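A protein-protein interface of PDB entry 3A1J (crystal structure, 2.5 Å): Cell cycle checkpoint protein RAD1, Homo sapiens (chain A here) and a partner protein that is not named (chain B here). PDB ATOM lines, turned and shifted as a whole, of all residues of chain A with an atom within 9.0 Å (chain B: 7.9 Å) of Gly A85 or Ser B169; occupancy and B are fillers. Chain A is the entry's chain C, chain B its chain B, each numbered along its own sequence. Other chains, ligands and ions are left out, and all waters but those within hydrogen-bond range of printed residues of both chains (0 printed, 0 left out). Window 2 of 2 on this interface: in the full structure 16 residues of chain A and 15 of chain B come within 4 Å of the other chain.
N of Val B170 lies close to O of Ile A83 (3.5 Å).
The side-chain amino group (NZ) of Lys B173 sits at hydrogen-bond distance from the backbone carbonyl oxygen (O) of Ser A82 (3.1 Å).
The side-chain amide nitrogen of Asn B176 is in hydrogen-bond range of the side-chain carboxylate of Asp A79 (3.4 Å).
OG1 of Thr A118 lies within hydrogen-bond range of OG1 of Thr B204 (2.8 Å).
The side-chain hydroxyl of Ser B169 lies within hydrogen-bond range of the backbone carbonyl oxygen of Lys B165 (3.1 Å).
The backbone carbonyl oxygen (O) of Leu B193 lies within hydrogen-bond range of the backbone NH (N) of Thr B204, 2.9 Å away.
The backbone carbonyl oxygen (O) of Leu A78 is in hydrogen-bond range of the side-chain hydroxyl (OG) of Ser A82 (3.1 Å).
Among the printed residues, merely in contact across the chains: Asp A79 with Lys B173 (3.5 Å), Ser A86 with Lys B173 (3.6 Å), Ile A83 with Ser B169 (3.6 Å), Gly A85 with Ser B169 (3.8 Å), Phe A84 with Ser B169 (3.8 Å) and Ile A83 with Lys B173 (3.8 Å).
Gly A85 touches just one residue of chain B: Ser B169.
Of chain A, only Ile A83, Phe A84 and Gly A85 come within 4 Å of Ser B169.
Printed residues of chain A within 4 Å of Asn B176: Asp A79 (3.4 Å).
Of the printed residues of chain B, Asp A79 touches Lys B173 (3.5 Å) and Asn B176 (3.4 Å).
Printed residues of chain A within 4 Å of Thr B204: Thr A118.
Thr B166 touches none of the printed residues of chain A.
Glu B172 touches none of the printed residues of chain A.
The nearest residue of chain B that does not touch Gly A85 is Lys B173 (4.7 Å).
The nearest printed residue of chain B that does not touch Ser A86 is Ser B169 (5.8 Å).
Hydrophobic or aromatic side chains of chain B that line the printed part of chain A: Val B170.
Along chain B the printed residues that touch a printed residue of chain A span positions 169 to 204.
Printed residues of chain A that touch a printed residue of chain B: Asp A79, Ser A82, Ile A83, Phe A84, Gly A85, Ser A86 and Thr A118.
Hydrophobic or aromatic side chains of chain A within 4 Å of the printed part of chain B: Ile A83.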
ATOM      1  N   VAL A  12     -12.140   8.580  18.522  1.00  0.00           N
ATOM      2  CA  VAL A  12     -12.529   8.381  17.116  1.00  0.00           C
ATOM      3  C   VAL A  12     -11.627   9.109  16.136  1.00  0.00           C
ATOM      4  O   VAL A  12     -11.394   8.626  15.028  1.00  0.00           O
ATOM      5  CB  VAL A  12     -13.971   8.849  16.794  1.00  0.00           C
ATOM      6  CG1 VAL A  12     -14.911   7.690  16.903  1.00  0.00           C
ATOM      7  CG2 VAL A  12     -14.388   9.999  17.692  1.00  0.00           C
ATOM      8  N   ARG A  13     -11.135  10.274  16.546  1.00  0.00           N
ATOM      9  CA  ARG A  13     -10.268  11.082  15.701  1.00  0.00           C
ATOM     10  C   ARG A  13      -9.026  10.345  15.204  1.00  0.00           C
ATOM     11  O   ARG A  13      -8.398  10.780  14.241  1.00  0.00           O
ATOM     12  CB  ARG A  13      -9.852  12.361  16.431  1.00  0.00           C
ATOM     13  CG  ARG A  13     -10.990  13.355  16.686  1.00  0.00           C
ATOM     14  CD  ARG A  13     -10.435  14.769  16.889  1.00  0.00           C
ATOM     15  NE  ARG A  13      -9.608  14.899  18.091  1.00  0.00           N
ATOM     16  CZ  ARG A  13     -10.089  15.143  19.307  1.00  0.00           C
ATOM     17  NH1 ARG A  13     -11.399  15.287  19.484  1.00  0.00           N
ATOM     18  NH2 ARG A  13      -9.263  15.249  20.345  1.00  0.00           N
ATOM     19  N   SER A  16     -11.228   8.963  12.187  1.00  0.00           N
ATOM     20  CA  SER A  16     -11.881   9.972  11.358  1.00  0.00           C
ATOM     21  C   SER A  16     -10.921  10.941  10.658  1.00  0.00           C
ATOM     22  O   SER A  16     -11.152  11.286   9.498  1.00  0.00           O
ATOM     23  CB  SER A  16     -12.933  10.759  12.163  1.00  0.00           C
ATOM     24  OG  SER A  16     -12.359  11.578  13.169  1.00  0.00           O
ATOM     25  N   LYS A  20     -10.558  11.404   6.565  1.00  0.00           N
ATOM     26  CA  LYS A  20     -10.891  12.666   5.909  1.00  0.00           C
ATOM     27  C   LYS A  20      -9.827  13.047   4.880  1.00  0.00           C
ATOM     28  O   LYS A  20     -10.099  13.788   3.937  1.00  0.00           O
ATOM     29  CB  LYS A  20     -11.063  13.782   6.946  1.00  0.00           C
ATOM     30  CG  LYS A  20     -12.484  13.869   7.499  1.00  0.00           C
ATOM     31  CD  LYS A  20     -12.508  14.311   8.959  1.00  0.00           C
ATOM     32  CE  LYS A  20     -11.781  15.632   9.147  1.00  0.00           C
ATOM     33  NZ  LYS A  20     -11.760  16.056  10.575  1.00  0.00           N
ATOM     34  N   LEU A  78     -18.120   9.040   7.701  1.00  0.00           N
ATOM     35  CA  LEU A  78     -17.508  10.205   8.329  1.00  0.00           C
ATOM     36  C   LEU A  78     -18.551  11.057   9.050  1.00  0.00           C
ATOM     37  O   LEU A  78     -18.252  11.665  10.081  1.00  0.00           O
ATOM     38  CB  LEU A  78     -16.761  11.047   7.289  1.00  0.00           C
ATOM     39  CG  LEU A  78     -15.401  10.470   6.868  1.00  0.00           C
ATOM     40  CD1 LEU A  78     -14.804  11.284   5.735  1.00  0.00           C
ATOM     41  CD2 LEU A  78     -14.468  10.461   8.076  1.00  0.00           C
ATOM     42  N   ASP A  79     -19.776  11.102   8.534  1.00  0.00           N
ATOM     43  CA  ASP A  79     -20.816  11.888   9.204  1.00  0.00           C
ATOM     44  C   ASP A  79     -21.096  11.314  10.590  1.00  0.00           C
ATOM     45  O   ASP A  79     -21.281  12.058  11.550  1.00  0.00           O
ATOM     46  CB  ASP A  79     -22.128  11.903   8.402  1.00  0.00           C
ATOM     47  CG  ASP A  79     -22.196  13.052   7.394  1.00  0.00           C
ATOM     48  OD1 ASP A  79     -21.788  14.184   7.758  1.00  0.00           O
ATOM     49  OD2 ASP A  79     -22.674  12.824   6.251  1.00  0.00           O
ATOM     50  N   CYS A  80     -21.133   9.988  10.678  1.00  0.00           N
ATOM     51  CA  CYS A  80     -21.387   9.296  11.931  1.00  0.00           C
ATOM     52  C   CYS A  80     -20.207   9.404  12.902  1.00  0.00           C
ATOM     53  O   CYS A  80     -20.393   9.585  14.108  1.00  0.00           O
ATOM     54  CB  CYS A  80     -21.686   7.821  11.653  1.00  0.00           C
ATOM     55  SG  CYS A  80     -23.218   7.518  10.726  1.00  0.00           S
ATOM     56  N   LEU A  81     -18.993   9.292  12.379  1.00  0.00           N
ATOM     57  CA  LEU A  81     -17.812   9.376  13.228  1.00  0.00           C
ATOM     58  C   LEU A  81     -17.670  10.748  13.875  1.00  0.00           C
ATOM     59  O   LEU A  81     -16.982  10.890  14.884  1.00  0.00           O
ATOM     60  CB  LEU A  81     -16.548   9.051  12.426  1.00  0.00           C
ATOM     61  CG  LEU A  81     -16.442   7.624  11.877  1.00  0.00           C
ATOM     62  CD1 LEU A  81     -15.168   7.492  11.059  1.00  0.00           C
ATOM     63  CD2 LEU A  81     -16.458   6.629  13.015  1.00  0.00           C
ATOM     64  N   SER A  82     -18.301  11.767  13.302  1.00  0.00           N
ATOM     65  CA  SER A  82     -18.215  13.096  13.902  1.00  0.00           C
ATOM     66  C   SER A  82     -19.603  13.562  14.329  1.00  0.00           C
ATOM     67  O   SER A  82     -19.894  14.761  14.354  1.00  0.00           O
ATOM     68  CB  SER A  82     -17.577  14.099  12.931  1.00  0.00           C
ATOM     69  OG  SER A  82     -18.339  14.267  11.748  1.00  0.00           O
ATOM     70  N   ILE A  83     -20.443  12.595  14.690  1.00  0.00           N
ATOM     71  CA  ILE A  83     -21.811  12.847  15.122  1.00  0.00           C
ATOM     72  C   ILE A  83     -21.882  13.800  16.313  1.00  0.00           C
ATOM     73  O   ILE A  83     -22.886  14.480  16.500  1.00  0.00           O
ATOM     74  CB  ILE A  83     -22.516  11.517  15.513  1.00  0.00           C
ATOM     75  CG1 ILE A  83     -24.035  11.678  15.452  1.00  0.00           C
ATOM     76  CG2 ILE A  83     -22.131  11.107  16.924  1.00  0.00           C
ATOM     77  CD1 ILE A  83     -24.592  11.648  14.039  1.00  0.00           C
ATOM     78  N   PHE A  84     -20.818  13.855  17.110  1.00  0.00           N
ATOM     79  CA  PHE A  84     -20.796  14.703  18.303  1.00  0.00           C
ATOM     80  C   PHE A  84     -20.134  16.070  18.159  1.00  0.00           C
ATOM     81  O   PHE A  84     -19.896  16.763  19.152  1.00  0.00           O
ATOM     82  CB  PHE A  84     -20.133  13.956  19.462  1.00  0.00           C
ATOM     83  CG  PHE A  84     -20.950  12.831  19.996  1.00  0.00           C
ATOM     84  CD1 PHE A  84     -22.243  13.057  20.461  1.00  0.00           C
ATOM     85  CD2 PHE A  84     -20.437  11.541  20.046  1.00  0.00           C
ATOM     86  CE1 PHE A  84     -23.019  12.011  20.970  1.00  0.00           C
ATOM     87  CE2 PHE A  84     -21.199  10.488  20.552  1.00  0.00           C
ATOM     88  CZ  PHE A  84     -22.497  10.726  21.015  1.00  0.00           C
ATOM     89  N   GLY A  85     -19.838  16.467  16.930  1.00  0.00           N
ATOM     90  CA  GLY A  85     -19.210  17.759  16.743  1.00  0.00           C
ATOM     91  C   GLY A  85     -17.821  17.620  16.174  1.00  0.00           C
ATOM     92  O   GLY A  85     -17.200  16.565  16.281  1.00  0.00           O
ATOM     93  N   SER A  86     -17.328  18.694  15.571  1.00  0.00           N
ATOM     94  CA  SER A  86     -16.011  18.668  14.967  1.00  0.00           C
ATOM     95  C   SER A  86     -15.044  19.622  15.664  1.00  0.00           C
ATOM     96  O   SER A  86     -13.939  19.871  15.178  1.00  0.00           O
ATOM     97  CB  SER A  86     -16.135  19.000  13.477  1.00  0.00           C
ATOM     98  OG  SER A  86     -17.016  18.091  12.829  1.00  0.00           O
ATOM     99  N   SER A  87     -15.462  20.145  16.813  1.00  0.00           N
ATOM    100  CA  SER A  87     -14.624  21.056  17.585  1.00  0.00           C
ATOM    101  C   SER A  87     -14.576  20.603  19.039  1.00  0.00           C
ATOM    102  O   SER A  87     -14.897  21.371  19.948  1.00  0.00           O
ATOM    103  CB  SER A  87     -15.185  22.476  17.523  1.00  0.00           C
ATOM    104  OG  SER A  87     -16.400  22.564  18.245  1.00  0.00           O
ATOM    105  N   PRO A  88     -14.175  19.343  19.282  1.00  0.00           N
ATOM    106  CA  PRO A  88     -14.106  18.834  20.655  1.00  0.00           C
ATOM    107  C   PRO A  88     -13.079  19.594  21.486  1.00  0.00           C
ATOM    108  O   PRO A  88     -12.149  20.196  20.948  1.00  0.00           O
ATOM    109  CB  PRO A  88     -13.722  17.366  20.464  1.00  0.00           C
ATOM    110  CG  PRO A  88     -14.235  17.046  19.081  1.00  0.00           C
ATOM    111  CD  PRO A  88     -13.839  18.280  18.319  1.00  0.00           C
ATOM    112  N   MET A  89     -13.252  19.553  22.801  1.00  0.00           N
ATOM    113  CA  MET A  89     -12.353  20.240  23.715  1.00  0.00           C
ATOM    114  C   MET A  89     -11.368  19.306  24.408  1.00  0.00           C
ATOM    115  O   MET A  89     -11.623  18.107  24.544  1.00  0.00           O
ATOM    116  CB  MET A  89     -13.169  20.994  24.761  1.00  0.00           C
ATOM    117  CG  MET A  89     -13.800  22.268  24.231  1.00  0.00           C
ATOM    118  SD  MET A  89     -12.438  23.531  23.688  1.00  0.00           S
ATOM    119  CE  MET A  89     -11.825  23.997  25.460  1.00  0.00           C
ATOM    120  N   THR A  92     -12.044  15.977  26.297  1.00  0.00           N
ATOM    121  CA  THR A  92     -13.371  15.528  25.901  1.00  0.00           C
ATOM    122  C   THR A  92     -13.281  14.606  24.702  1.00  0.00           C
ATOM    123  O   THR A  92     -13.306  15.057  23.561  1.00  0.00           O
ATOM    124  CB  THR A  92     -14.267  16.713  25.537  1.00  0.00           C
ATOM    125  OG1 THR A  92     -14.279  17.652  26.623  1.00  0.00           O
ATOM    126  CG2 THR A  92     -15.694  16.230  25.254  1.00  0.00           C
ATOM    127  N   THR A  94     -14.471  11.154  22.320  1.00  0.00           N
ATOM    128  CA  THR A  94     -15.603  10.373  21.843  1.00  0.00           C
ATOM    129  C   THR A  94     -15.005   9.003  21.539  1.00  0.00           C
ATOM    130  O   THR A  94     -14.126   8.884  20.683  1.00  0.00           O
ATOM    131  CB  THR A  94     -16.195  10.945  20.539  1.00  0.00           C
ATOM    132  OG1 THR A  94     -16.789  12.220  20.799  1.00  0.00           O
ATOM    133  CG2 THR A  94     -17.256  10.010  19.979  1.00  0.00           C
ATOM    134  N   GLU A 113     -19.960  10.041  24.017  1.00  0.00           N
ATOM    135  CA  GLU A 113     -19.294  11.248  24.471  1.00  0.00           C
ATOM    136  C   GLU A 113     -20.056  11.745  25.683  1.00  0.00           C
ATOM    137  O   GLU A 113     -21.262  11.964  25.619  1.00  0.00           O
ATOM    138  CB  GLU A 113     -19.290  12.337  23.388  1.00  0.00           C
ATOM    139  CG  GLU A 113     -18.877  13.693  23.964  1.00  0.00           C
ATOM    140  CD  GLU A 113     -19.055  14.866  23.009  1.00  0.00           C
ATOM    141  OE1 GLU A 113     -18.231  15.016  22.070  1.00  0.00           O
ATOM    142  OE2 GLU A 113     -20.021  15.637  23.211  1.00  0.00           O
ATOM    143  N   THR A 118     -24.325   7.048  20.618  1.00  0.00           N
ATOM    144  CA  THR A 118     -24.923   7.017  19.289  1.00  0.00           C
ATOM    145  C   THR A 118     -24.673   5.654  18.653  1.00  0.00           C
ATOM    146  O   THR A 118     -23.550   5.148  18.680  1.00  0.00           O
ATOM    147  CB  THR A 118     -24.346   8.108  18.342  1.00  0.00           C
ATOM    148  OG1 THR A 118     -24.674   9.417  18.839  1.00  0.00           O
ATOM    149  CG2 THR A 118     -24.934   7.946  16.942  1.00  0.00           C
ATOM    150  N   VAL B 163     -27.927  19.145  26.839  1.00  0.00           N
ATOM    151  CA  VAL B 163     -27.153  20.305  26.387  1.00  0.00           C
ATOM    152  C   VAL B 163     -27.496  20.559  24.926  1.00  0.00           C
ATOM    153  O   VAL B 163     -27.270  19.696  24.077  1.00  0.00           O
ATOM    154  CB  VAL B 163     -25.639  20.051  26.482  1.00  0.00           C
ATOM    155  CG1 VAL B 163     -24.881  21.340  26.208  1.00  0.00           C
ATOM    156  CG2 VAL B 163     -25.290  19.507  27.850  1.00  0.00           C
ATOM    157  N   LEU B 164     -28.027  21.743  24.634  1.00  0.00           N
ATOM    158  CA  LEU B 164     -28.431  22.087  23.274  1.00  0.00           C
ATOM    159  C   LEU B 164     -27.317  22.049  22.227  1.00  0.00           C
ATOM    160  O   LEU B 164     -27.542  21.606  21.104  1.00  0.00           O
ATOM    161  CB  LEU B 164     -29.127  23.448  23.278  1.00  0.00           C
ATOM    162  CG  LEU B 164     -30.378  23.500  24.172  1.00  0.00           C
ATOM    163  CD1 LEU B 164     -31.057  24.845  24.000  1.00  0.00           C
ATOM    164  CD2 LEU B 164     -31.350  22.377  23.805  1.00  0.00           C
ATOM    165  N   LYS B 165     -26.118  22.503  22.585  1.00  0.00           N
ATOM    166  CA  LYS B 165     -24.995  22.461  21.645  1.00  0.00           C
ATOM    167  C   LYS B 165     -24.766  21.032  21.151  1.00  0.00           C
ATOM    168  O   LYS B 165     -24.529  20.812  19.965  1.00  0.00           O
ATOM    169  CB  LYS B 165     -23.706  22.964  22.302  1.00  0.00           C
ATOM    170  CG  LYS B 165     -23.729  24.434  22.676  1.00  0.00           C
ATOM    171  CD  LYS B 165     -22.352  24.910  23.139  1.00  0.00           C
ATOM    172  CE  LYS B 165     -22.251  26.435  23.128  1.00  0.00           C
ATOM    173  NZ  LYS B 165     -20.899  26.896  23.537  1.00  0.00           N
ATOM    174  N   THR B 166     -24.833  20.067  22.067  1.00  0.00           N
ATOM    175  CA  THR B 166     -24.630  18.665  21.721  1.00  0.00           C
ATOM    176  C   THR B 166     -25.741  18.182  20.798  1.00  0.00           C
ATOM    177  O   THR B 166     -25.480  17.480  19.822  1.00  0.00           O
ATOM    178  CB  THR B 166     -24.589  17.770  22.978  1.00  0.00           C
ATOM    179  OG1 THR B 166     -23.546  18.209  23.854  1.00  0.00           O
ATOM    180  CG2 THR B 166     -24.322  16.330  22.593  1.00  0.00           C
ATOM    181  N   MET B 167     -26.979  18.554  21.104  1.00  0.00           N
ATOM    182  CA  MET B 167     -28.109  18.165  20.265  1.00  0.00           C
ATOM    183  C   MET B 167     -27.942  18.745  18.871  1.00  0.00           C
ATOM    184  O   MET B 167     -28.209  18.077  17.868  1.00  0.00           O
ATOM    185  CB  MET B 167     -29.414  18.689  20.838  1.00  0.00           C
ATOM    186  CG  MET B 167     -30.194  17.692  21.640  1.00  0.00           C
ATOM    187  SD  MET B 167     -31.802  18.526  22.282  1.00  0.00           S
ATOM    188  CE  MET B 167     -32.971  18.173  20.780  1.00  0.00           C
ATOM    189  N   LYS B 168     -27.508  20.002  18.823  1.00  0.00           N
ATOM    190  CA  LYS B 168     -27.303  20.704  17.565  1.00  0.00           C
ATOM    191  C   LYS B 168     -26.342  19.924  16.684  1.00  0.00           C
ATOM    192  O   LYS B 168     -26.635  19.654  15.518  1.00  0.00           O
ATOM    193  CB  LYS B 168     -26.755  22.109  17.837  1.00  0.00           C
ATOM    194  CG  LYS B 168     -26.500  22.967  16.606  1.00  0.00           C
ATOM    195  CD  LYS B 168     -26.104  24.378  17.044  1.00  0.00           C
ATOM    196  CE  LYS B 168     -25.731  25.275  15.868  1.00  0.00           C
ATOM    197  NZ  LYS B 168     -24.454  24.866  15.223  1.00  0.00           N
ATOM    198  N   SER B 169     -25.200  19.547  17.246  1.00  0.00           N
ATOM    199  CA  SER B 169     -24.205  18.797  16.497  1.00  0.00           C
ATOM    200  C   SER B 169     -24.795  17.525  15.910  1.00  0.00           C
ATOM    201  O   SER B 169     -24.630  17.235  14.726  1.00  0.00           O
ATOM    202  CB  SER B 169     -23.040  18.433  17.406  1.00  0.00           C
ATOM    203  OG  SER B 169     -22.499  19.598  17.998  1.00  0.00           O
ATOM    204  N   VAL B 170     -25.493  16.772  16.751  1.00  0.00           N
ATOM    205  CA  VAL B 170     -26.100  15.522  16.334  1.00  0.00           C
ATOM    206  C   VAL B 170     -27.169  15.700  15.241  1.00  0.00           C
ATOM    207  O   VAL B 170     -27.121  15.009  14.218  1.00  0.00           O
ATOM    208  CB  VAL B 170     -26.682  14.775  17.579  1.00  0.00           C
ATOM    209  CG1 VAL B 170     -27.441  13.531  17.163  1.00  0.00           C
ATOM    210  CG2 VAL B 170     -25.544  14.398  18.526  1.00  0.00           C
ATOM    211  N   VAL B 171     -28.126  16.610  15.421  1.00  0.00           N
ATOM    212  CA  VAL B 171     -29.145  16.774  14.381  1.00  0.00           C
ATOM    213  C   VAL B 171     -28.533  17.401  13.128  1.00  0.00           C
ATOM    214  O   VAL B 171     -29.024  17.213  12.020  1.00  0.00           O
ATOM    215  CB  VAL B 171     -30.342  17.622  14.855  1.00  0.00           C
ATOM    216  CG1 VAL B 171     -30.569  17.402  16.331  1.00  0.00           C
ATOM    217  CG2 VAL B 171     -30.125  19.074  14.527  1.00  0.00           C
ATOM    218  N   GLU B 172     -27.447  18.136  13.315  1.00  0.00           N
ATOM    219  CA  GLU B 172     -26.744  18.759  12.200  1.00  0.00           C
ATOM    220  C   GLU B 172     -26.321  17.643  11.246  1.00  0.00           C
ATOM    221  O   GLU B 172     -26.652  17.653  10.062  1.00  0.00           O
ATOM    222  CB  GLU B 172     -25.501  19.479  12.724  1.00  0.00           C
ATOM    223  CG  GLU B 172     -25.402  20.934  12.356  1.00  0.00           C
ATOM    224  CD  GLU B 172     -24.537  21.709  13.336  1.00  0.00           C
ATOM    225  OE1 GLU B 172     -23.359  21.326  13.541  1.00  0.00           O
ATOM    226  OE2 GLU B 172     -25.041  22.704  13.906  1.00  0.00           O
ATOM    227  N   LYS B 173     -25.589  16.675  11.793  1.00  0.00           N
ATOM    228  CA  LYS B 173     -25.095  15.536  11.035  1.00  0.00           C
ATOM    229  C   LYS B 173     -26.198  14.601  10.550  1.00  0.00           C
ATOM    230  O   LYS B 173     -26.116  14.069   9.446  1.00  0.00           O
ATOM    231  CB  LYS B 173     -24.081  14.766  11.887  1.00  0.00           C
ATOM    232  CG  LYS B 173     -22.814  15.560  12.167  1.00  0.00           C
ATOM    233  CD  LYS B 173     -21.984  15.681  10.899  1.00  0.00           C
ATOM    234  CE  LYS B 173     -21.063  16.881  10.948  1.00  0.00           C
ATOM    235  NZ  LYS B 173     -20.376  16.999  12.256  1.00  0.00           N
ATOM    236  N   MET B 174     -27.228  14.393  11.362  1.00  0.00           N
ATOM    237  CA  MET B 174     -28.315  13.520  10.948  1.00  0.00           C
ATOM    238  C   MET B 174     -29.009  14.108   9.731  1.00  0.00           C
ATOM    239  O   MET B 174     -29.439  13.381   8.834  1.00  0.00           O
ATOM    240  CB  MET B 174     -29.332  13.345  12.071  1.00  0.00           C
ATOM    241  CG  MET B 174     -28.807  12.589  13.269  1.00  0.00           C
ATOM    242  SD  MET B 174     -30.199  12.166  14.552  1.00  0.00           S
ATOM    243  CE  MET B 174     -30.229  13.832  15.491  1.00  0.00           C
ATOM    244  N   LYS B 175     -29.120  15.434   9.709  1.00  0.00           N
ATOM    245  CA  LYS B 175     -29.766  16.138   8.605  1.00  0.00           C
ATOM    246  C   LYS B 175     -29.056  15.861   7.286  1.00  0.00           C
ATOM    247  O   LYS B 175     -29.669  15.915   6.217  1.00  0.00           O
ATOM    248  CB  LYS B 175     -29.782  17.645   8.877  1.00  0.00           C
ATOM    249  CG  LYS B 175     -30.389  18.469   7.765  1.00  0.00           C
ATOM    250  CD  LYS B 175     -30.146  19.935   8.027  1.00  0.00           C
ATOM    251  CE  LYS B 175     -30.714  20.816   6.928  1.00  0.00           C
ATOM    252  NZ  LYS B 175     -30.457  22.253   7.234  1.00  0.00           N
ATOM    253  N   ASN B 176     -27.761  15.572   7.364  1.00  0.00           N
ATOM    254  CA  ASN B 176     -27.005  15.269   6.166  1.00  0.00           C
ATOM    255  C   ASN B 176     -27.425  13.910   5.621  1.00  0.00           C
ATOM    256  O   ASN B 176     -27.161  13.596   4.468  1.00  0.00           O
ATOM    257  CB  ASN B 176     -25.505  15.253   6.458  1.00  0.00           C
ATOM    258  CG  ASN B 176     -24.949  16.632   6.757  1.00  0.00           C
ATOM    259  OD1 ASN B 176     -25.340  17.620   6.128  1.00  0.00           O
ATOM    260  ND2 ASN B 176     -24.015  16.708   7.709  1.00  0.00           N
ATOM    261  N   LEU B 193     -32.931  10.598  19.709  1.00  0.00           N
ATOM    262  CA  LEU B 193     -33.084  11.256  18.428  1.00  0.00           C
ATOM    263  C   LEU B 193     -32.828  10.107  17.457  1.00  0.00           C
ATOM    264  O   LEU B 193     -31.858   9.361  17.607  1.00  0.00           O
ATOM    265  CB  LEU B 193     -32.049  12.374  18.259  1.00  0.00           C
ATOM    266  CG  LEU B 193     -32.314  13.595  19.148  1.00  0.00           C
ATOM    267  CD1 LEU B 193     -31.238  14.652  18.953  1.00  0.00           C
ATOM    268  CD2 LEU B 193     -33.695  14.144  18.816  1.00  0.00           C
ATOM    269  N   THR B 204     -29.317   8.409  18.619  1.00  0.00           N
ATOM    270  CA  THR B 204     -28.525   8.985  19.698  1.00  0.00           C
ATOM    271  C   THR B 204     -29.333   8.923  20.985  1.00  0.00           C
ATOM    272  O   THR B 204     -30.447   9.450  21.061  1.00  0.00           O
ATOM    273  CB  THR B 204     -28.121  10.439  19.389  1.00  0.00           C
ATOM    274  OG1 THR B 204     -27.179  10.441  18.313  1.00  0.00           O
ATOM    275  CG2 THR B 204     -27.474  11.083  20.593  1.00  0.00           C
ATOM    276  N   LEU B 239     -33.534  21.766  13.653  1.00  0.00           N
ATOM    277  CA  LEU B 239     -32.210  22.368  13.497  1.00  0.00           C
ATOM    278  C   LEU B 239     -32.357  23.869  13.662  1.00  0.00           C
ATOM    279  O   LEU B 239     -31.581  24.515  14.363  1.00  0.00           O
ATOM    280  CB  LEU B 239     -31.636  22.078  12.107  1.00  0.00           C
ATOM    281  CG  LEU B 239     -30.142  21.762  12.030  1.00  0.00           C
ATOM    282  CD1 LEU B 239     -29.657  21.995  10.618  1.00  0.00           C
ATOM    283  CD2 LEU B 239     -29.367  22.632  12.998  1.00  0.00           C
ATOM    284  N   LEU B 242     -32.796  24.890  17.313  1.00  0.00           N
ATOM    285  CA  LEU B 242     -31.536  24.720  18.039  1.00  0.00           C
ATOM    286  C   LEU B 242     -30.480  25.719  17.573  1.00  0.00           C
ATOM    287  O   LEU B 242     -29.704  26.234  18.373  1.00  0.00           O
ATOM    288  CB  LEU B 242     -31.015  23.289  17.857  1.00  0.00           C
ATOM    289  CG  LEU B 242     -31.878  22.191  18.483  1.00  0.00           C
ATOM    290  CD1 LEU B 242     -31.446  20.828  17.963  1.00  0.00           C
ATOM    291  CD2 LEU B 242     -31.775  22.260  19.999  1.00  0.00           C
